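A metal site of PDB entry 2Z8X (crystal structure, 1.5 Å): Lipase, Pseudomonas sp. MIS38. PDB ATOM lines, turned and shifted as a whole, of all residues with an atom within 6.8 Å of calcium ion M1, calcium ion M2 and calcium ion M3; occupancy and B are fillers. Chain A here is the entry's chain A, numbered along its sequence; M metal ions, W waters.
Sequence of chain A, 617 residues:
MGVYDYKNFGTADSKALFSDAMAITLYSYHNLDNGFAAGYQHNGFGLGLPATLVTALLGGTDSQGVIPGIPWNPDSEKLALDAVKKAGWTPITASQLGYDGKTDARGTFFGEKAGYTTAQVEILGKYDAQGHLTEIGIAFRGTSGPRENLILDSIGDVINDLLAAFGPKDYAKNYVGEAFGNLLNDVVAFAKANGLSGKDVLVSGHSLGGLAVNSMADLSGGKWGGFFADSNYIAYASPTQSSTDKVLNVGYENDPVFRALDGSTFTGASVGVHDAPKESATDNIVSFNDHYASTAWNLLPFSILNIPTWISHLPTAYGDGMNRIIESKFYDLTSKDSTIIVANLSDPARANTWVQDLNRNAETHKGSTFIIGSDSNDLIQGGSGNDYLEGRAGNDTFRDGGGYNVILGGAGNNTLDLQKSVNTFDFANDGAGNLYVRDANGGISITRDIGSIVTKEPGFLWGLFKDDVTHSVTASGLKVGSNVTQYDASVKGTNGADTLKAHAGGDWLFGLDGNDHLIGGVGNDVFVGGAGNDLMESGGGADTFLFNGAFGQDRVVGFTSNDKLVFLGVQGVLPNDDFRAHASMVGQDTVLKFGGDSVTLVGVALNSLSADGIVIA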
ATOM      1  N   GLY A 493      22.222   8.043 -11.009  1.00  0.00           N
ATOM      2  CA  GLY A 493      23.633   7.997 -10.696  1.00  0.00           C
ATOM      3  C   GLY A 493      23.984   6.849  -9.782  1.00  0.00           C
ATOM      4  O   GLY A 493      23.359   5.772  -9.829  1.00  0.00           O
ATOM      5  N   THR A 494      25.012   7.060  -8.971  1.00  0.00           N
ATOM      6  CA  THR A 494      25.483   6.090  -7.995  1.00  0.00           C
ATOM      7  C   THR A 494      25.653   6.825  -6.673  1.00  0.00           C
ATOM      8  O   THR A 494      25.433   8.053  -6.589  1.00  0.00           O
ATOM      9  CB  THR A 494      26.861   5.497  -8.405  1.00  0.00           C
ATOM     10  OG1 THR A 494      27.883   6.502  -8.303  1.00  0.00           O
ATOM     11  CG2 THR A 494      26.819   4.958  -9.829  1.00  0.00           C
ATOM     12  N   ASN A 495      26.082   6.131  -5.634  1.00  0.00           N
ATOM     13  CA  ASN A 495      26.344   6.827  -4.382  1.00  0.00           C
ATOM     14  C   ASN A 495      27.725   7.479  -4.297  1.00  0.00           C
ATOM     15  O   ASN A 495      28.091   8.011  -3.280  1.00  0.00           O
ATOM     16  CB  ASN A 495      26.085   5.913  -3.187  1.00  0.00           C
ATOM     17  CG  ASN A 495      24.608   5.713  -2.899  1.00  0.00           C
ATOM     18  OD1 ASN A 495      23.799   6.610  -3.036  1.00  0.00           O
ATOM     19  ND2 ASN A 495      24.267   4.516  -2.477  1.00  0.00           N
ATOM     20  N   GLY A 496      28.441   7.440  -5.405  1.00  0.00           N
ATOM     21  CA  GLY A 496      29.660   8.249  -5.562  1.00  0.00           C
ATOM     22  C   GLY A 496      29.380   9.502  -6.378  1.00  0.00           C
ATOM     23  O   GLY A 496      28.223   9.798  -6.691  1.00  0.00           O
ATOM     24  N   ALA A 497      30.429  10.259  -6.706  1.00  0.00           N
ATOM     25  CA  ALA A 497      30.274  11.473  -7.515  1.00  0.00           C
ATOM     26  C   ALA A 497      30.034  11.123  -8.987  1.00  0.00           C
ATOM     27  O   ALA A 497      30.834  10.409  -9.606  1.00  0.00           O
ATOM     28  CB  ALA A 497      31.498  12.362  -7.361  1.00  0.00           C
ATOM     29  N   ASP A 498      28.926  11.628  -9.525  1.00  0.00           N
ATOM     30  CA  ASP A 498      28.537  11.361 -10.918  1.00  0.00           C
ATOM     31  C   ASP A 498      28.341  12.641 -11.695  1.00  0.00           C
ATOM     32  O   ASP A 498      27.962  13.662 -11.130  1.00  0.00           O
ATOM     33  CB  ASP A 498      27.202  10.618 -10.995  1.00  0.00           C
ATOM     34  CG  ASP A 498      27.098   9.474 -10.013  1.00  0.00           C
ATOM     35  OD1 ASP A 498      27.870   8.508 -10.159  1.00  0.00           O
ATOM     36  OD2 ASP A 498      26.216   9.554  -9.114  1.00  0.00           O
ATOM     37  N   LEU A 500      25.699  13.480 -14.607  1.00  0.00           N
ATOM     38  CA  LEU A 500      24.520  12.935 -15.292  1.00  0.00           C
ATOM     39  C   LEU A 500      24.031  13.979 -16.276  1.00  0.00           C
ATOM     40  O   LEU A 500      23.931  15.155 -15.941  1.00  0.00           O
ATOM     41  CB  LEU A 500      23.399  12.616 -14.293  1.00  0.00           C
ATOM     42  CG  LEU A 500      23.712  11.662 -13.144  1.00  0.00           C
ATOM     43  CD1 LEU A 500      22.428  11.410 -12.361  1.00  0.00           C
ATOM     44  CD2 LEU A 500      24.319  10.362 -13.654  1.00  0.00           C
ATOM     45  N   PHE A 510      18.645  11.705 -11.014  1.00  0.00           N
ATOM     46  CA  PHE A 510      18.788  11.258  -9.628  1.00  0.00           C
ATOM     47  C   PHE A 510      20.255  11.073  -9.265  1.00  0.00           C
ATOM     48  O   PHE A 510      20.861  10.044  -9.570  1.00  0.00           O
ATOM     49  CB  PHE A 510      18.049   9.927  -9.425  1.00  0.00           C
ATOM     50  CG  PHE A 510      16.566  10.009  -9.644  1.00  0.00           C
ATOM     51  CD1 PHE A 510      15.755  10.728  -8.770  1.00  0.00           C
ATOM     52  CD2 PHE A 510      15.977   9.311 -10.690  1.00  0.00           C
ATOM     53  CE1 PHE A 510      14.380  10.767  -8.949  1.00  0.00           C
ATOM     54  CE2 PHE A 510      14.615   9.347 -10.875  1.00  0.00           C
ATOM     55  CZ  PHE A 510      13.805  10.080 -10.005  1.00  0.00           C
ATOM     56  N   GLY A 511      20.826  12.063  -8.581  1.00  0.00           N
ATOM     57  CA  GLY A 511      22.235  12.025  -8.244  1.00  0.00           C
ATOM     58  C   GLY A 511      22.583  10.987  -7.189  1.00  0.00           C
ATOM     59  O   GLY A 511      23.679  10.453  -7.184  1.00  0.00           O
ATOM     60  N   LEU A 512      21.634  10.733  -6.285  1.00  0.00           N
ATOM     61  CA  LEU A 512      21.886   9.892  -5.104  1.00  0.00           C
ATOM     62  C   LEU A 512      23.037  10.468  -4.256  1.00  0.00           C
ATOM     63  O   LEU A 512      23.322  11.675  -4.325  1.00  0.00           O
ATOM     64  CB  LEU A 512      22.152   8.439  -5.516  1.00  0.00           C
ATOM     65  CG  LEU A 512      21.153   7.800  -6.498  1.00  0.00           C
ATOM     66  CD1 LEU A 512      21.596   6.372  -6.868  1.00  0.00           C
ATOM     67  CD2 LEU A 512      19.704   7.836  -5.965  1.00  0.00           C
ATOM     68  N   ASP A 513      23.710   9.642  -3.449  1.00  0.00           N
ATOM     69  CA  ASP A 513      24.763  10.174  -2.578  1.00  0.00           C
ATOM     70  C   ASP A 513      25.966  10.689  -3.378  1.00  0.00           C
ATOM     71  O   ASP A 513      26.089  10.405  -4.571  1.00  0.00           O
ATOM     72  CB  ASP A 513      25.236   9.128  -1.561  1.00  0.00           C
ATOM     73  CG  ASP A 513      24.135   8.648  -0.616  1.00  0.00           C
ATOM     74  OD1 ASP A 513      23.002   9.192  -0.602  1.00  0.00           O
ATOM     75  OD2 ASP A 513      24.423   7.685   0.134  1.00  0.00           O
ATOM     76  N   GLY A 514      26.818  11.457  -2.722  1.00  0.00           N
ATOM     77  CA  GLY A 514      28.017  11.993  -3.357  1.00  0.00           C
ATOM     78  C   GLY A 514      27.774  13.353  -3.984  1.00  0.00           C
ATOM     79  O   GLY A 514      26.627  13.771  -4.167  1.00  0.00           O
ATOM     80  N   ASN A 515      28.855  14.037  -4.324  1.00  0.00           N
ATOM     81  CA  ASN A 515      28.769  15.384  -4.898  1.00  0.00           C
ATOM     82  C   ASN A 515      28.636  15.288  -6.403  1.00  0.00           C
ATOM     83  O   ASN A 515      29.621  15.047  -7.120  1.00  0.00           O
ATOM     84  CB  ASN A 515      30.006  16.203  -4.532  1.00  0.00           C
ATOM     85  CG  ASN A 515      30.213  16.359  -3.027  1.00  0.00           C
ATOM     86  OD1 ASN A 515      29.298  16.189  -2.224  1.00  0.00           O
ATOM     87  ND2 ASN A 515      31.436  16.686  -2.647  1.00  0.00           N
ATOM     88  N   ASP A 516      27.417  15.508  -6.887  1.00  0.00           N
ATOM     89  CA  ASP A 516      27.102  15.229  -8.272  1.00  0.00           C
ATOM     90  C   ASP A 516      27.037  16.475  -9.143  1.00  0.00           C
ATOM     91  O   ASP A 516      26.909  17.585  -8.644  1.00  0.00           O
ATOM     92  CB  ASP A 516      25.794  14.444  -8.355  1.00  0.00           C
ATOM     93  CG  ASP A 516      25.864  13.163  -7.550  1.00  0.00           C
ATOM     94  OD1 ASP A 516      26.788  12.371  -7.806  1.00  0.00           O
ATOM     95  OD2 ASP A 516      25.019  12.967  -6.663  1.00  0.00           O
ATOM     96  N   LEU A 518      24.891  17.609 -12.271  1.00  0.00           N
ATOM     97  CA  LEU A 518      23.686  17.285 -13.019  1.00  0.00           C
ATOM     98  C   LEU A 518      23.458  18.288 -14.125  1.00  0.00           C
ATOM     99  O   LEU A 518      23.179  19.462 -13.849  1.00  0.00           O
ATOM    100  CB  LEU A 518      22.472  17.248 -12.071  1.00  0.00           C
ATOM    101  CG  LEU A 518      22.137  15.931 -11.361  1.00  0.00           C
ATOM    102  CD1 LEU A 518      23.345  15.173 -10.866  1.00  0.00           C
ATOM    103  CD2 LEU A 518      21.100  16.123 -10.267  1.00  0.00           C
ATOM    104  N   VAL A 528      17.065  15.895  -8.768  1.00  0.00           N
ATOM    105  CA  VAL A 528      17.102  15.416  -7.395  1.00  0.00           C
ATOM    106  C   VAL A 528      18.566  15.126  -7.064  1.00  0.00           C
ATOM    107  O   VAL A 528      19.062  13.998  -7.266  1.00  0.00           O
ATOM    108  CB  VAL A 528      16.211  14.177  -7.183  1.00  0.00           C
ATOM    109  CG1 VAL A 528      16.108  13.890  -5.691  1.00  0.00           C
ATOM    110  CG2 VAL A 528      14.823  14.417  -7.750  1.00  0.00           C
ATOM    111  N   GLY A 529      19.265  16.141  -6.569  1.00  0.00           N
ATOM    112  CA  GLY A 529      20.690  16.009  -6.265  1.00  0.00           C
ATOM    113  C   GLY A 529      20.943  14.934  -5.216  1.00  0.00           C
ATOM    114  O   GLY A 529      21.971  14.242  -5.262  1.00  0.00           O
ATOM    115  N   GLY A 530      20.016  14.822  -4.278  1.00  0.00           N
ATOM    116  CA  GLY A 530      20.164  13.885  -3.153  1.00  0.00           C
ATOM    117  C   GLY A 530      21.192  14.358  -2.146  1.00  0.00           C
ATOM    118  O   GLY A 530      21.555  15.541  -2.101  1.00  0.00           O
ATOM    119  N   ALA A 531      21.664  13.433  -1.313  1.00  0.00           N
ATOM    120  CA  ALA A 531      22.737  13.753  -0.378  1.00  0.00           C
ATOM    121  C   ALA A 531      23.975  14.224  -1.139  1.00  0.00           C
ATOM    122  O   ALA A 531      24.135  13.955  -2.346  1.00  0.00           O
ATOM    123  CB  ALA A 531      23.068  12.551   0.478  1.00  0.00           C
ATOM    124  N   GLY A 532      24.836  14.955  -0.431  1.00  0.00           N
ATOM    125  CA  GLY A 532      26.041  15.490  -1.022  1.00  0.00           C
ATOM    126  C   GLY A 532      25.799  16.877  -1.585  1.00  0.00           C
ATOM    127  O   GLY A 532      24.668  17.379  -1.609  1.00  0.00           O
ATOM    128  N   ASN A 533      26.883  17.495  -2.042  1.00  0.00           N
ATOM    129  CA  ASN A 533      26.851  18.875  -2.514  1.00  0.00           C
ATOM    130  C   ASN A 533      26.809  18.828  -4.025  1.00  0.00           C
ATOM    131  O   ASN A 533      27.818  18.532  -4.671  1.00  0.00           O
ATOM    132  CB  ASN A 533      28.095  19.634  -2.029  1.00  0.00           C
ATOM    133  CG  ASN A 533      28.211  19.669  -0.511  1.00  0.00           C
ATOM    134  OD1 ASN A 533      27.231  19.444   0.214  1.00  0.00           O
ATOM    135  ND2 ASN A 533      29.414  19.956  -0.026  1.00  0.00           N
ATOM    136  N   ASP A 534      25.637  19.112  -4.577  1.00  0.00           N
ATOM    137  CA  ASP A 534      25.403  18.877  -5.986  1.00  0.00           C
ATOM    138  C   ASP A 534      25.349  20.168  -6.780  1.00  0.00           C
ATOM    139  O   ASP A 534      24.771  21.159  -6.327  1.00  0.00           O
ATOM    140  CB  ASP A 534      24.117  18.073  -6.173  1.00  0.00           C
ATOM    141  CG  ASP A 534      24.112  16.791  -5.370  1.00  0.00           C
ATOM    142  OD1 ASP A 534      24.878  15.858  -5.699  1.00  0.00           O
ATOM    143  OD2 ASP A 534      23.351  16.711  -4.396  1.00  0.00           O
ATOM    144  N   MET A 536      23.876  21.702 -10.136  1.00  0.00           N
ATOM    145  CA  MET A 536      22.747  21.359 -10.996  1.00  0.00           C
ATOM    146  C   MET A 536      22.460  22.508 -11.960  1.00  0.00           C
ATOM    147  O   MET A 536      22.182  23.627 -11.528  1.00  0.00           O
ATOM    148  CB  MET A 536      21.529  21.041 -10.118  1.00  0.00           C
ATOM    149  CG  MET A 536      21.839  19.882  -9.153  1.00  0.00           C
ATOM    150  SD  MET A 536      20.471  19.430  -8.104  1.00  0.00           S
ATOM    151  CE  MET A 536      20.609  20.641  -6.812  1.00  0.00           C
ATOM    152  N   PHE A 547      14.367  19.085  -3.127  1.00  0.00           N
ATOM    153  CA  PHE A 547      15.287  19.000  -1.986  1.00  0.00           C
ATOM    154  C   PHE A 547      14.574  18.336  -0.822  1.00  0.00           C
ATOM    155  O   PHE A 547      13.519  18.789  -0.402  1.00  0.00           O
ATOM    156  CB  PHE A 547      15.793  20.397  -1.592  1.00  0.00           C
ATOM    157  CG  PHE A 547      16.392  21.163  -2.726  1.00  0.00           C
ATOM    158  CD1 PHE A 547      17.736  20.996  -3.068  1.00  0.00           C
ATOM    159  CD2 PHE A 547      15.605  22.029  -3.487  1.00  0.00           C
ATOM    160  CE1 PHE A 547      18.282  21.683  -4.139  1.00  0.00           C
ATOM    161  CE2 PHE A 547      16.152  22.716  -4.558  1.00  0.00           C
ATOM    162  CZ  PHE A 547      17.494  22.545  -4.886  1.00  0.00           C
ATOM    163  N   ALA A 550      18.599  15.712   4.562  1.00  0.00           N
ATOM    164  CA  ALA A 550      19.861  16.416   4.753  1.00  0.00           C
ATOM    165  C   ALA A 550      20.518  16.544   3.375  1.00  0.00           C
ATOM    166  O   ALA A 550      21.413  15.760   3.015  1.00  0.00           O
ATOM    167  CB  ALA A 550      20.752  15.660   5.734  1.00  0.00           C
ATOM    168  N   PHE A 551      20.051  17.523   2.621  1.00  0.00           N
ATOM    169  CA  PHE A 551      20.332  17.581   1.188  1.00  0.00           C
ATOM    170  C   PHE A 551      21.671  18.221   0.812  1.00  0.00           C
ATOM    171  O   PHE A 551      22.036  18.225  -0.360  1.00  0.00           O
ATOM    172  CB  PHE A 551      19.167  18.215   0.401  1.00  0.00           C
ATOM    173  CG  PHE A 551      18.889  19.644   0.755  1.00  0.00           C
ATOM    174  CD1 PHE A 551      17.887  19.968   1.664  1.00  0.00           C
ATOM    175  CD2 PHE A 551      19.612  20.669   0.161  1.00  0.00           C
ATOM    176  CE1 PHE A 551      17.635  21.311   1.987  1.00  0.00           C
ATOM    177  CE2 PHE A 551      19.376  21.998   0.491  1.00  0.00           C
ATOM    178  CZ  PHE A 551      18.380  22.314   1.398  1.00  0.00           C
ATOM    179  N   GLY A 552      22.400  18.741   1.807  1.00  0.00           N
ATOM    180  CA  GLY A 552      23.752  19.253   1.551  1.00  0.00           C
ATOM    181  C   GLY A 552      23.802  20.706   1.119  1.00  0.00           C
ATOM    182  O   GLY A 552      22.874  21.467   1.397  1.00  0.00           O
ATOM    183  N   GLN A 553      24.920  21.080   0.489  1.00  0.00           N
ATOM    184  CA  GLN A 553      25.120  22.456   0.023  1.00  0.00           C
ATOM    185  C   GLN A 553      25.148  22.408  -1.494  1.00  0.00           C
ATOM    186  O   GLN A 553      26.174  22.069  -2.104  1.00  0.00           O
ATOM    187  CB  GLN A 553      26.426  23.071   0.543  1.00  0.00           C
ATOM    188  CG  GLN A 553      26.870  22.569   1.918  1.00  0.00           C
ATOM    189  CD  GLN A 553      25.862  22.863   3.016  1.00  0.00           C
ATOM    190  OE1 GLN A 553      25.631  22.026   3.889  1.00  0.00           O
ATOM    191  NE2 GLN A 553      25.286  24.054   2.988  1.00  0.00           N
ATOM    192  N   ASP A 554      24.020  22.752  -2.100  1.00  0.00           N
ATOM    193  CA  ASP A 554      23.836  22.615  -3.540  1.00  0.00           C
ATOM    194  C   ASP A 554      23.984  23.963  -4.230  1.00  0.00           C
ATOM    195  O   ASP A 554      23.771  24.992  -3.635  1.00  0.00           O
ATOM    196  CB  ASP A 554      22.438  22.074  -3.821  1.00  0.00           C
ATOM    197  CG  ASP A 554      22.210  20.682  -3.275  1.00  0.00           C
ATOM    198  OD1 ASP A 554      23.175  19.875  -3.229  1.00  0.00           O
ATOM    199  OD2 ASP A 554      21.043  20.400  -2.936  1.00  0.00           O
ATOM    200  N   SER A 598      21.849  23.986   2.351  1.00  0.00           N
ATOM    201  CA  SER A 598      21.636  25.225   1.606  1.00  0.00           C
ATOM    202  C   SER A 598      21.541  25.009   0.109  1.00  0.00           C
ATOM    203  O   SER A 598      22.095  24.039  -0.430  1.00  0.00           O
ATOM    204  CB  SER A 598      22.756  26.234   1.875  1.00  0.00           C
ATOM    205  OG  SER A 598      23.993  25.771   1.337  1.00  0.00           O
HETATM  206 CA    CA M   1      25.971  10.301  -6.893  1.00  0.00          CA
HETATM  207 CA    CA M   2      24.243  13.864  -4.651  1.00  0.00          CA
HETATM  208 CA    CA M   3      22.443  17.667  -2.475  1.00  0.00          CA
HETATM  209  O   HOH W   1      20.296  17.951  -3.470  1.00  0.00           O
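Water W1 bridges the side-chain carboxylate of Asp 554 (2.6 Å) and the backbone NH of Gly 530 (3.2 Å).
Calcium ion M1 is bound by O of Gly 511, 2.3 Å away.
Calcium ion M1 is bound by the backbone carbonyl oxygen (O) of Gly 496, 2.3 Å away.
The backbone carbonyl oxygen (O) of Asp 513 is bound to calcium ion M1.
Calcium ion M1 is bound by O of Thr 494 (2.3 Å).
Calcium ion M1 is bound by OD2 of Asp 498.
Calcium ion M1 is bound by OD1 of Asp 516 (2.4 Å).
Calcium ion M1 is bound by the side-chain carboxylate (OD2) of Asp 516 (2.8 Å).
Calcium ion M1 has seven donor atoms within binding distance.
The nearest printed residue that does not touch calcium ion M2 is Gly 511 (4.2 Å).
The backbone carbonyl oxygen (O) of Ala 531 is bound to calcium ion M2.
OD2 of Asp 516 binds calcium ion M2, 2.3 Å away.
Calcium ion M2 is bound by OD1 of Asp 534.
Calcium ion M2 is bound by the backbone carbonyl oxygen (O) of Gly 529.
O of Leu 512 is bound to calcium ion M2, 2.4 Å away.
O of Gly 514 is bound to calcium ion M2 (2.4 Å).
Slightly farther from calcium ion M2 lies the side-chain carboxylate (OD2) of Asp 534 (3.0 Å).
Of the 30 residues printed, 7 come within 4 Å of calcium ion M1.
Within 4 Å of calcium ion M3: Gly 530, Ala 531, Gly 532, Asp 534, Phe 551 and Asp 554.
Along chain A the residues within 4 Å of calcium ion M3 span positions 530 to 554.
The nearest printed residue that does not touch calcium ion M3 is Gly 529 (4.2 Å).
Calcium ion M3 is bound by the backbone carbonyl oxygen (O) of Phe 551 (2.2 Å), the side-chain carboxylate (OD2) of Asp 534 (2.3 Å), the backbone carbonyl oxygen (O) of Gly 530 (2.3 Å), water W1 (2.4 Å), the backbone carbonyl oxygen (O) of Gly 532 (2.4 Å) and the side-chain carboxylate (OD1) of Asp 554 (2.4 Å).
Slightly farther from calcium ion M3 lies the side-chain carboxylate (OD2) of Asp 554 (3.1 Å).
The backbone carbonyl oxygen (O) of Val 528 lies within hydrogen-bond range of the backbone NH (N) of Gly 511 (2.9 Å).
The backbone NH (N) of Gly 496 sits at hydrogen-bond distance from the side-chain hydroxyl (OG1) of Thr 494.
The backbone NH (N) of Asp 513 lies within hydrogen-bond range of the side-chain amide oxygen (OD1) of Asn 495, 3.1 Å away.
The backbone carbonyl oxygen (O) of Ser 598 is in hydrogen-bond range of the backbone NH (N) of Asp 554, 2.9 Å away.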
